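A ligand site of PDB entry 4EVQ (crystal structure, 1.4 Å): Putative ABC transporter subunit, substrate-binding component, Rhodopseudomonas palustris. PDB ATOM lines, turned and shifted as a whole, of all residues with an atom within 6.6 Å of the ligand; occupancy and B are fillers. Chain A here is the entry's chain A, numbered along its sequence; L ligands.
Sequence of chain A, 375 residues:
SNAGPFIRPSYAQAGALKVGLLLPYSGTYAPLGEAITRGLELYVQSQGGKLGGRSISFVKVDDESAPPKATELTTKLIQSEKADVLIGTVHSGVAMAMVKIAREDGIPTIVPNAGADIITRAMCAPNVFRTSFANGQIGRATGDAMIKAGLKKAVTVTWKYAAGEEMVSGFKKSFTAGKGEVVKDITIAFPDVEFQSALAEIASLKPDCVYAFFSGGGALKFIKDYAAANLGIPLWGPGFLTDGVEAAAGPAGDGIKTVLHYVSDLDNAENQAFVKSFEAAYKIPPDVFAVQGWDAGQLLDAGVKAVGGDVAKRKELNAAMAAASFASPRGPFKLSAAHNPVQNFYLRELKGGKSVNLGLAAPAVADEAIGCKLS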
ATOM      1  N   TYR A  29     -14.483 -17.828  27.211  1.00  0.00           N
ATOM      2  CA  TYR A  29     -15.068 -19.110  26.922  1.00  0.00           C
ATOM      3  C   TYR A  29     -15.131 -20.052  28.134  1.00  0.00           C
ATOM      4  O   TYR A  29     -15.405 -21.232  27.998  1.00  0.00           O
ATOM      5  CB  TYR A  29     -14.319 -19.740  25.760  1.00  0.00           C
ATOM      6  CG  TYR A  29     -14.605 -19.136  24.378  1.00  0.00           C
ATOM      7  CD1 TYR A  29     -15.803 -18.532  24.057  1.00  0.00           C
ATOM      8  CD2 TYR A  29     -13.671 -19.247  23.356  1.00  0.00           C
ATOM      9  CE1 TYR A  29     -16.058 -18.079  22.771  1.00  0.00           C
ATOM     10  CE2 TYR A  29     -13.899 -18.777  22.085  1.00  0.00           C
ATOM     11  CZ  TYR A  29     -15.097 -18.196  21.784  1.00  0.00           C
ATOM     12  OH  TYR A  29     -15.380 -17.748  20.512  1.00  0.00           O
ATOM     13  N   LEU A  32     -18.043 -22.438  28.266  1.00  0.00           N
ATOM     14  CA  LEU A  32     -17.943 -23.553  27.315  1.00  0.00           C
ATOM     15  C   LEU A  32     -17.004 -24.626  27.885  1.00  0.00           C
ATOM     16  O   LEU A  32     -17.289 -25.810  27.790  1.00  0.00           O
ATOM     17  CB  LEU A  32     -17.428 -23.071  25.952  1.00  0.00           C
ATOM     18  CG  LEU A  32     -18.408 -22.310  25.056  1.00  0.00           C
ATOM     19  CD1 LEU A  32     -18.919 -21.005  25.675  1.00  0.00           C
ATOM     20  CD2 LEU A  32     -17.771 -22.046  23.710  1.00  0.00           C
ATOM     21  N   THR A  89      -9.530 -28.440  22.350  1.00  0.00           N
ATOM     22  CA  THR A  89     -10.010 -27.428  23.263  1.00  0.00           C
ATOM     23  C   THR A  89     -11.188 -26.690  22.608  1.00  0.00           C
ATOM     24  O   THR A  89     -11.790 -27.213  21.648  1.00  0.00           O
ATOM     25  CB  THR A  89      -8.875 -26.509  23.647  1.00  0.00           C
ATOM     26  OG1 THR A  89      -9.357 -25.508  24.588  1.00  0.00           O
ATOM     27  CG2 THR A  89      -8.278 -25.794  22.444  1.00  0.00           C
ATOM     28  N   VAL A  90     -11.526 -25.499  23.091  1.00  0.00           N
ATOM     29  CA  VAL A  90     -12.604 -24.672  22.543  1.00  0.00           C
ATOM     30  C   VAL A  90     -12.220 -23.765  21.422  1.00  0.00           C
ATOM     31  O   VAL A  90     -12.850 -23.783  20.371  1.00  0.00           O
ATOM     32  CB  VAL A  90     -13.256 -23.857  23.688  1.00  0.00           C
ATOM     33  CG1 VAL A  90     -14.232 -22.803  23.164  1.00  0.00           C
ATOM     34  CG2 VAL A  90     -13.992 -24.798  24.652  1.00  0.00           C
ATOM     35  N   HIS A  91     -11.196 -22.948  21.615  1.00  0.00           N
ATOM     36  CA  HIS A  91     -10.789 -21.901  20.667  1.00  0.00           C
ATOM     37  C   HIS A  91      -9.945 -22.494  19.540  1.00  0.00           C
ATOM     38  O   HIS A  91      -8.977 -23.193  19.795  1.00  0.00           O
ATOM     39  CB  HIS A  91     -10.015 -20.849  21.479  1.00  0.00           C
ATOM     40  CG  HIS A  91      -9.576 -19.631  20.723  1.00  0.00           C
ATOM     41  ND1 HIS A  91      -8.550 -19.647  19.799  1.00  0.00           N
ATOM     42  CD2 HIS A  91      -9.920 -18.334  20.871  1.00  0.00           C
ATOM     43  CE1 HIS A  91      -8.321 -18.421  19.372  1.00  0.00           C
ATOM     44  NE2 HIS A  91      -9.151 -17.601  19.997  1.00  0.00           N
ATOM     45  N   SER A  92     -10.340 -22.228  18.304  1.00  0.00           N
ATOM     46  CA  SER A  92      -9.689 -22.834  17.157  1.00  0.00           C
ATOM     47  C   SER A  92      -8.224 -22.505  17.018  1.00  0.00           C
ATOM     48  O   SER A  92      -7.469 -23.328  16.535  1.00  0.00           O
ATOM     49  CB  SER A  92     -10.374 -22.407  15.864  1.00  0.00           C
ATOM     50  OG  SER A  92     -11.538 -23.150  15.584  1.00  0.00           O
ATOM     51  N   GLY A  93      -7.815 -21.301  17.395  1.00  0.00           N
ATOM     52  CA  GLY A  93      -6.396 -20.974  17.325  1.00  0.00           C
ATOM     53  C   GLY A  93      -5.565 -21.784  18.333  1.00  0.00           C
ATOM     54  O   GLY A  93      -4.474 -22.255  17.974  1.00  0.00           O
ATOM     55  N   ASN A 113     -14.569 -29.348  20.842  1.00  0.00           N
ATOM     56  CA  ASN A 113     -15.306 -28.196  20.322  1.00  0.00           C
ATOM     57  C   ASN A 113     -14.656 -27.519  19.106  1.00  0.00           C
ATOM     58  O   ASN A 113     -15.276 -27.414  18.055  1.00  0.00           O
ATOM     59  CB  ASN A 113     -15.535 -27.071  21.367  1.00  0.00           C
ATOM     60  CG  ASN A 113     -16.404 -25.968  20.787  1.00  0.00           C
ATOM     61  OD1 ASN A 113     -17.597 -26.186  20.573  1.00  0.00           O
ATOM     62  ND2 ASN A 113     -15.782 -24.839  20.427  1.00  0.00           N
ATOM     63  N   ALA A 114     -13.414 -27.053  19.247  1.00  0.00           N
ATOM     64  CA  ALA A 114     -12.784 -26.214  18.218  1.00  0.00           C
ATOM     65  C   ALA A 114     -13.095 -26.701  16.828  1.00  0.00           C
ATOM     66  O   ALA A 114     -12.797 -27.851  16.478  1.00  0.00           O
ATOM     67  CB  ALA A 114     -11.276 -26.134  18.410  1.00  0.00           C
ATOM     68  N   GLY A 115     -13.635 -25.845  16.014  1.00  0.00           N
ATOM     69  CA  GLY A 115     -14.057 -26.186  14.662  1.00  0.00           C
ATOM     70  C   GLY A 115     -13.036 -26.038  13.591  1.00  0.00           C
ATOM     71  O   GLY A 115     -13.353 -26.306  12.419  1.00  0.00           O
ATOM     72  N   ALA A 116     -11.807 -25.673  13.946  1.00  0.00           N
ATOM     73  CA  ALA A 116     -10.799 -25.330  12.942  1.00  0.00           C
ATOM     74  C   ALA A 116     -10.830 -26.313  11.787  1.00  0.00           C
ATOM     75  O   ALA A 116     -10.630 -27.526  11.992  1.00  0.00           O
ATOM     76  CB  ALA A 116      -9.422 -25.292  13.595  1.00  0.00           C
ATOM     77  N   PHE A 133     -17.684 -30.498  15.276  1.00  0.00           N
ATOM     78  CA  PHE A 133     -18.084 -30.018  13.956  1.00  0.00           C
ATOM     79  C   PHE A 133     -16.865 -29.386  13.331  1.00  0.00           C
ATOM     80  O   PHE A 133     -15.879 -29.102  14.028  1.00  0.00           O
ATOM     81  CB  PHE A 133     -19.244 -29.005  14.056  1.00  0.00           C
ATOM     82  CG  PHE A 133     -18.824 -27.797  14.810  1.00  0.00           C
ATOM     83  CD1 PHE A 133     -18.793 -27.820  16.183  1.00  0.00           C
ATOM     84  CD2 PHE A 133     -18.271 -26.703  14.158  1.00  0.00           C
ATOM     85  CE1 PHE A 133     -18.239 -26.790  16.887  1.00  0.00           C
ATOM     86  CE2 PHE A 133     -17.747 -25.643  14.901  1.00  0.00           C
ATOM     87  CZ  PHE A 133     -17.707 -25.721  16.243  1.00  0.00           C
ATOM     88  N   ASN A 135     -15.885 -25.823  11.198  1.00  0.00           N
ATOM     89  CA  ASN A 135     -16.376 -24.445  11.017  1.00  0.00           C
ATOM     90  C   ASN A 135     -16.970 -24.213   9.654  1.00  0.00           C
ATOM     91  O   ASN A 135     -18.052 -23.645   9.534  1.00  0.00           O
ATOM     92  CB  ASN A 135     -15.187 -23.494  11.190  1.00  0.00           C
ATOM     93  CG  ASN A 135     -14.739 -23.342  12.641  1.00  0.00           C
ATOM     94  OD1 ASN A 135     -15.506 -23.485  13.578  1.00  0.00           O
ATOM     95  ND2 ASN A 135     -13.475 -22.990  12.798  1.00  0.00           N
ATOM     96  N   TYR A 161     -10.920 -13.844  14.433  1.00  0.00           N
ATOM     97  CA  TYR A 161      -9.990 -14.931  14.642  1.00  0.00           C
ATOM     98  C   TYR A 161     -10.474 -16.090  13.775  1.00  0.00           C
ATOM     99  O   TYR A 161     -11.544 -16.022  13.171  1.00  0.00           O
ATOM    100  CB  TYR A 161      -9.810 -15.302  16.122  1.00  0.00           C
ATOM    101  CG  TYR A 161     -10.845 -16.245  16.719  1.00  0.00           C
ATOM    102  CD1 TYR A 161     -12.065 -15.757  17.099  1.00  0.00           C
ATOM    103  CD2 TYR A 161     -10.577 -17.590  16.973  1.00  0.00           C
ATOM    104  CE1 TYR A 161     -13.008 -16.574  17.701  1.00  0.00           C
ATOM    105  CE2 TYR A 161     -11.497 -18.394  17.560  1.00  0.00           C
ATOM    106  CZ  TYR A 161     -12.719 -17.897  17.926  1.00  0.00           C
ATOM    107  OH  TYR A 161     -13.643 -18.702  18.527  1.00  0.00           O
ATOM    108  N   ALA A 162      -9.723 -17.192  13.784  1.00  0.00           N
ATOM    109  CA  ALA A 162      -9.948 -18.281  12.827  1.00  0.00           C
ATOM    110  C   ALA A 162     -11.362 -18.789  12.771  1.00  0.00           C
ATOM    111  O   ALA A 162     -11.865 -19.071  11.704  1.00  0.00           O
ATOM    112  CB  ALA A 162      -8.962 -19.438  13.079  1.00  0.00           C
ATOM    113  N   ALA A 163     -11.994 -18.990  13.919  1.00  0.00           N
ATOM    114  CA  ALA A 163     -13.287 -19.610  13.890  1.00  0.00           C
ATOM    115  C   ALA A 163     -14.304 -18.705  13.240  1.00  0.00           C
ATOM    116  O   ALA A 163     -15.152 -19.168  12.458  1.00  0.00           O
ATOM    117  CB  ALA A 163     -13.754 -20.050  15.262  1.00  0.00           C
ATOM    118  N   GLY A 164     -14.262 -17.432  13.583  1.00  0.00           N
ATOM    119  CA  GLY A 164     -15.188 -16.494  12.960  1.00  0.00           C
ATOM    120  C   GLY A 164     -14.910 -16.397  11.472  1.00  0.00           C
ATOM    121  O   GLY A 164     -15.844 -16.445  10.657  1.00  0.00           O
ATOM    122  N   MET A 167     -16.172 -19.759   9.749  1.00  0.00           N
ATOM    123  CA  MET A 167     -17.619 -19.887   9.706  1.00  0.00           C
ATOM    124  C   MET A 167     -18.250 -18.858   8.783  1.00  0.00           C
ATOM    125  O   MET A 167     -19.246 -19.157   8.120  1.00  0.00           O
ATOM    126  CB  MET A 167     -18.210 -19.805  11.096  1.00  0.00           C
ATOM    127  CG  MET A 167     -17.984 -21.050  11.927  1.00  0.00           C
ATOM    128  SD  MET A 167     -18.983 -21.119  13.553  1.00  0.00           S
ATOM    129  CE  MET A 167     -17.568 -21.108  14.776  1.00  0.00           C
ATOM    130  N   PHE A 213     -21.590 -14.864  14.281  1.00  0.00           N
ATOM    131  CA  PHE A 213     -20.965 -15.865  15.139  1.00  0.00           C
ATOM    132  C   PHE A 213     -20.344 -15.177  16.346  1.00  0.00           C
ATOM    133  O   PHE A 213     -19.369 -14.408  16.208  1.00  0.00           O
ATOM    134  CB  PHE A 213     -19.918 -16.778  14.478  1.00  0.00           C
ATOM    135  CG  PHE A 213     -19.064 -17.539  15.504  1.00  0.00           C
ATOM    136  CD1 PHE A 213     -19.651 -18.468  16.323  1.00  0.00           C
ATOM    137  CD2 PHE A 213     -17.721 -17.241  15.712  1.00  0.00           C
ATOM    138  CE1 PHE A 213     -18.936 -19.103  17.326  1.00  0.00           C
ATOM    139  CE2 PHE A 213     -17.002 -17.872  16.746  1.00  0.00           C
ATOM    140  CZ  PHE A 213     -17.635 -18.796  17.540  1.00  0.00           C
ATOM    141  N   PHE A 214     -20.936 -15.472  17.496  1.00  0.00           N
ATOM    142  CA  PHE A 214     -20.364 -15.157  18.831  1.00  0.00           C
ATOM    143  C   PHE A 214     -20.782 -16.345  19.683  1.00  0.00           C
ATOM    144  O   PHE A 214     -21.642 -17.155  19.304  1.00  0.00           O
ATOM    145  CB  PHE A 214     -20.930 -13.853  19.407  1.00  0.00           C
ATOM    146  CG  PHE A 214     -20.564 -12.657  18.624  1.00  0.00           C
ATOM    147  CD1 PHE A 214     -19.303 -12.137  18.679  1.00  0.00           C
ATOM    148  CD2 PHE A 214     -21.469 -12.071  17.752  1.00  0.00           C
ATOM    149  CE1 PHE A 214     -18.905 -11.098  17.889  1.00  0.00           C
ATOM    150  CE2 PHE A 214     -21.098 -11.048  16.968  1.00  0.00           C
ATOM    151  CZ  PHE A 214     -19.829 -10.535  17.010  1.00  0.00           C
ATOM    152  N   SER A 215     -20.160 -16.500  20.855  1.00  0.00           N
ATOM    153  CA  SER A 215     -20.499 -17.581  21.736  1.00  0.00           C
ATOM    154  C   SER A 215     -20.110 -17.184  23.165  1.00  0.00           C
ATOM    155  O   SER A 215     -19.220 -16.379  23.346  1.00  0.00           O
ATOM    156  CB  SER A 215     -19.725 -18.836  21.253  1.00  0.00           C
ATOM    157  OG  SER A 215     -19.978 -19.965  22.005  1.00  0.00           O
ATOM    158  N   GLY A 216     -20.832 -17.684  24.146  1.00  0.00           N
ATOM    159  CA  GLY A 216     -20.577 -17.347  25.544  1.00  0.00           C
ATOM    160  C   GLY A 216     -21.229 -16.048  25.907  1.00  0.00           C
ATOM    161  O   GLY A 216     -22.220 -15.615  25.314  1.00  0.00           O
ATOM    162  N   PHE A 240     -24.089 -21.815  18.071  1.00  0.00           N
ATOM    163  CA  PHE A 240     -23.265 -21.280  19.153  1.00  0.00           C
ATOM    164  C   PHE A 240     -23.739 -19.905  19.590  1.00  0.00           C
ATOM    165  O   PHE A 240     -23.476 -19.485  20.713  1.00  0.00           O
ATOM    166  CB  PHE A 240     -21.788 -21.241  18.748  1.00  0.00           C
ATOM    167  CG  PHE A 240     -21.352 -22.445  18.003  1.00  0.00           C
ATOM    168  CD1 PHE A 240     -21.338 -23.677  18.629  1.00  0.00           C
ATOM    169  CD2 PHE A 240     -21.033 -22.374  16.655  1.00  0.00           C
ATOM    170  CE1 PHE A 240     -21.001 -24.799  17.926  1.00  0.00           C
ATOM    171  CE2 PHE A 240     -20.728 -23.539  15.947  1.00  0.00           C
ATOM    172  CZ  PHE A 240     -20.723 -24.730  16.575  1.00  0.00           C
ATOM    173  N   LEU A 241     -24.392 -19.168  18.686  1.00  0.00           N
ATOM    174  CA  LEU A 241     -24.853 -17.805  18.971  1.00  0.00           C
ATOM    175  C   LEU A 241     -25.875 -17.823  20.091  1.00  0.00           C
ATOM    176  O   LEU A 241     -25.946 -16.854  20.824  1.00  0.00           O
ATOM    177  CB  LEU A 241     -25.486 -17.264  17.694  1.00  0.00           C
ATOM    178  CG  LEU A 241     -26.041 -15.841  17.772  1.00  0.00           C
ATOM    179  CD1 LEU A 241     -24.952 -14.838  18.079  1.00  0.00           C
ATOM    180  CD2 LEU A 241     -26.771 -15.489  16.468  1.00  0.00           C
ATOM    181  N   VAL A 288     -24.945 -27.679  23.558  1.00  0.00           N
ATOM    182  CA  VAL A 288     -24.151 -28.446  22.584  1.00  0.00           C
ATOM    183  C   VAL A 288     -22.771 -28.753  23.111  1.00  0.00           C
ATOM    184  O   VAL A 288     -22.206 -29.799  22.771  1.00  0.00           O
ATOM    185  CB  VAL A 288     -24.094 -27.716  21.204  1.00  0.00           C
ATOM    186  CG1 VAL A 288     -23.293 -26.421  21.270  1.00  0.00           C
ATOM    187  CG2 VAL A 288     -23.607 -28.654  20.088  1.00  0.00           C
ATOM    188  N   PHE A 289     -22.180 -27.859  23.913  1.00  0.00           N
ATOM    189  CA  PHE A 289     -20.842 -28.063  24.424  1.00  0.00           C
ATOM    190  C   PHE A 289     -20.836 -29.212  25.385  1.00  0.00           C
ATOM    191  O   PHE A 289     -19.919 -30.074  25.348  1.00  0.00           O
ATOM    192  CB  PHE A 289     -20.351 -26.738  25.045  1.00  0.00           C
ATOM    193  CG  PHE A 289     -20.530 -25.575  24.116  1.00  0.00           C
ATOM    194  CD1 PHE A 289     -19.739 -25.451  23.000  1.00  0.00           C
ATOM    195  CD2 PHE A 289     -21.461 -24.592  24.373  1.00  0.00           C
ATOM    196  CE1 PHE A 289     -19.926 -24.410  22.094  1.00  0.00           C
ATOM    197  CE2 PHE A 289     -21.639 -23.541  23.528  1.00  0.00           C
ATOM    198  CZ  PHE A 289     -20.891 -23.445  22.384  1.00  0.00           C
HETATM  199  C1  LIG L   1     -13.841 -22.059  17.954  1.00  0.00           C
HETATM  200  O1  LIG L   1     -12.954 -21.205  18.212  1.00  0.00           O
HETATM  201  O2  LIG L   1     -13.630 -23.053  17.151  1.00  0.00           O
HETATM  202  C2  LIG L   1     -15.182 -21.995  18.549  1.00  0.00           C
HETATM  203  C3  LIG L   1     -15.367 -21.314  19.760  1.00  0.00           C
HETATM  204  C4  LIG L   1     -16.633 -21.242  20.316  1.00  0.00           C
HETATM  205  C5  LIG L   1     -17.689 -21.811  19.670  1.00  0.00           C
HETATM  206  C6  LIG L   1     -17.536 -22.497  18.487  1.00  0.00           C
HETATM  207  C7  LIG L   1     -16.286 -22.567  17.949  1.00  0.00           C
HETATM  208  O3  LIG L   1     -18.924 -21.733  20.197  1.00  0.00           O
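O1 of the ligand lies close to O of Val 90 (3.4 Å). Merely in contact with the ligand: Phe 240, Ala 163, His 91, Asn 113, Phe 289, Ala 114, Tyr 29, Leu 32, Phe 213, Met 167 and Phe 133. Hydrophobic or aromatic side chains that line the ligand: Tyr 29, Leu 32, Val 90, Phe 133, Tyr 161, Ala 163, Met 167, Phe 213, Phe 240 and Phe 289. Within 4 Å of the ligand: Tyr 29, Leu 32, Val 90, His 91, Ser 92, Asn 113, Ala 114, Gly 115, Phe 133, Tyr 161, Ala 163, Met 167, Phe 213, Ser 215, Phe 240 and Phe 289.
The side-chain hydroxyl (OH) of Tyr 161 lies within hydrogen-bond range of an oxygen (O1) of the ligand. An oxygen (O1) of the ligand lies within hydrogen-bond range of the backbone NH (N) of Ser 92, 2.8 Å away. OG of Ser 92 is in hydrogen-bond range of O2 of the ligand (2.6 Å). An oxygen (O3) of the ligand sits at hydrogen-bond distance from the side-chain hydroxyl (OG) of Ser 215 (2.7 Å). The backbone NH (N) of Gly 115 is in hydrogen-bond range of an oxygen (O2) of the ligand (3.0 Å).
The side-chain hydroxyl (OH) of Tyr 29 lies within hydrogen-bond range of the side-chain hydroxyl (OH) of Tyr 161, at 2.8 Å. OG of Ser 92 lies within hydrogen-bond range of N of Gly 115 (3.4 Å). The side-chain hydroxyl (OG) of Ser 92 sits at hydrogen-bond distance from the side-chain amide nitrogen (ND2) of Asn 135, at 3.4 Å. The backbone NH (N) of Ala 116 sits at hydrogen-bond distance from the side-chain hydroxyl (OG) of Ser 92 (3.0 Å). N of Asn 135 sits at hydrogen-bond distance from O of Gly 115 (2.9 Å). O of Val 90 is in hydrogen-bond range of ND2 of Asn 113, at 3.1 Å. A ring nitrogen (ND1) of His 91 lies within hydrogen-bond range of the backbone NH of Gly 93 (3.0 Å). The backbone NH of Ala 114 is in hydrogen-bond range of the backbone carbonyl oxygen of Thr 89 (2.9 Å).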
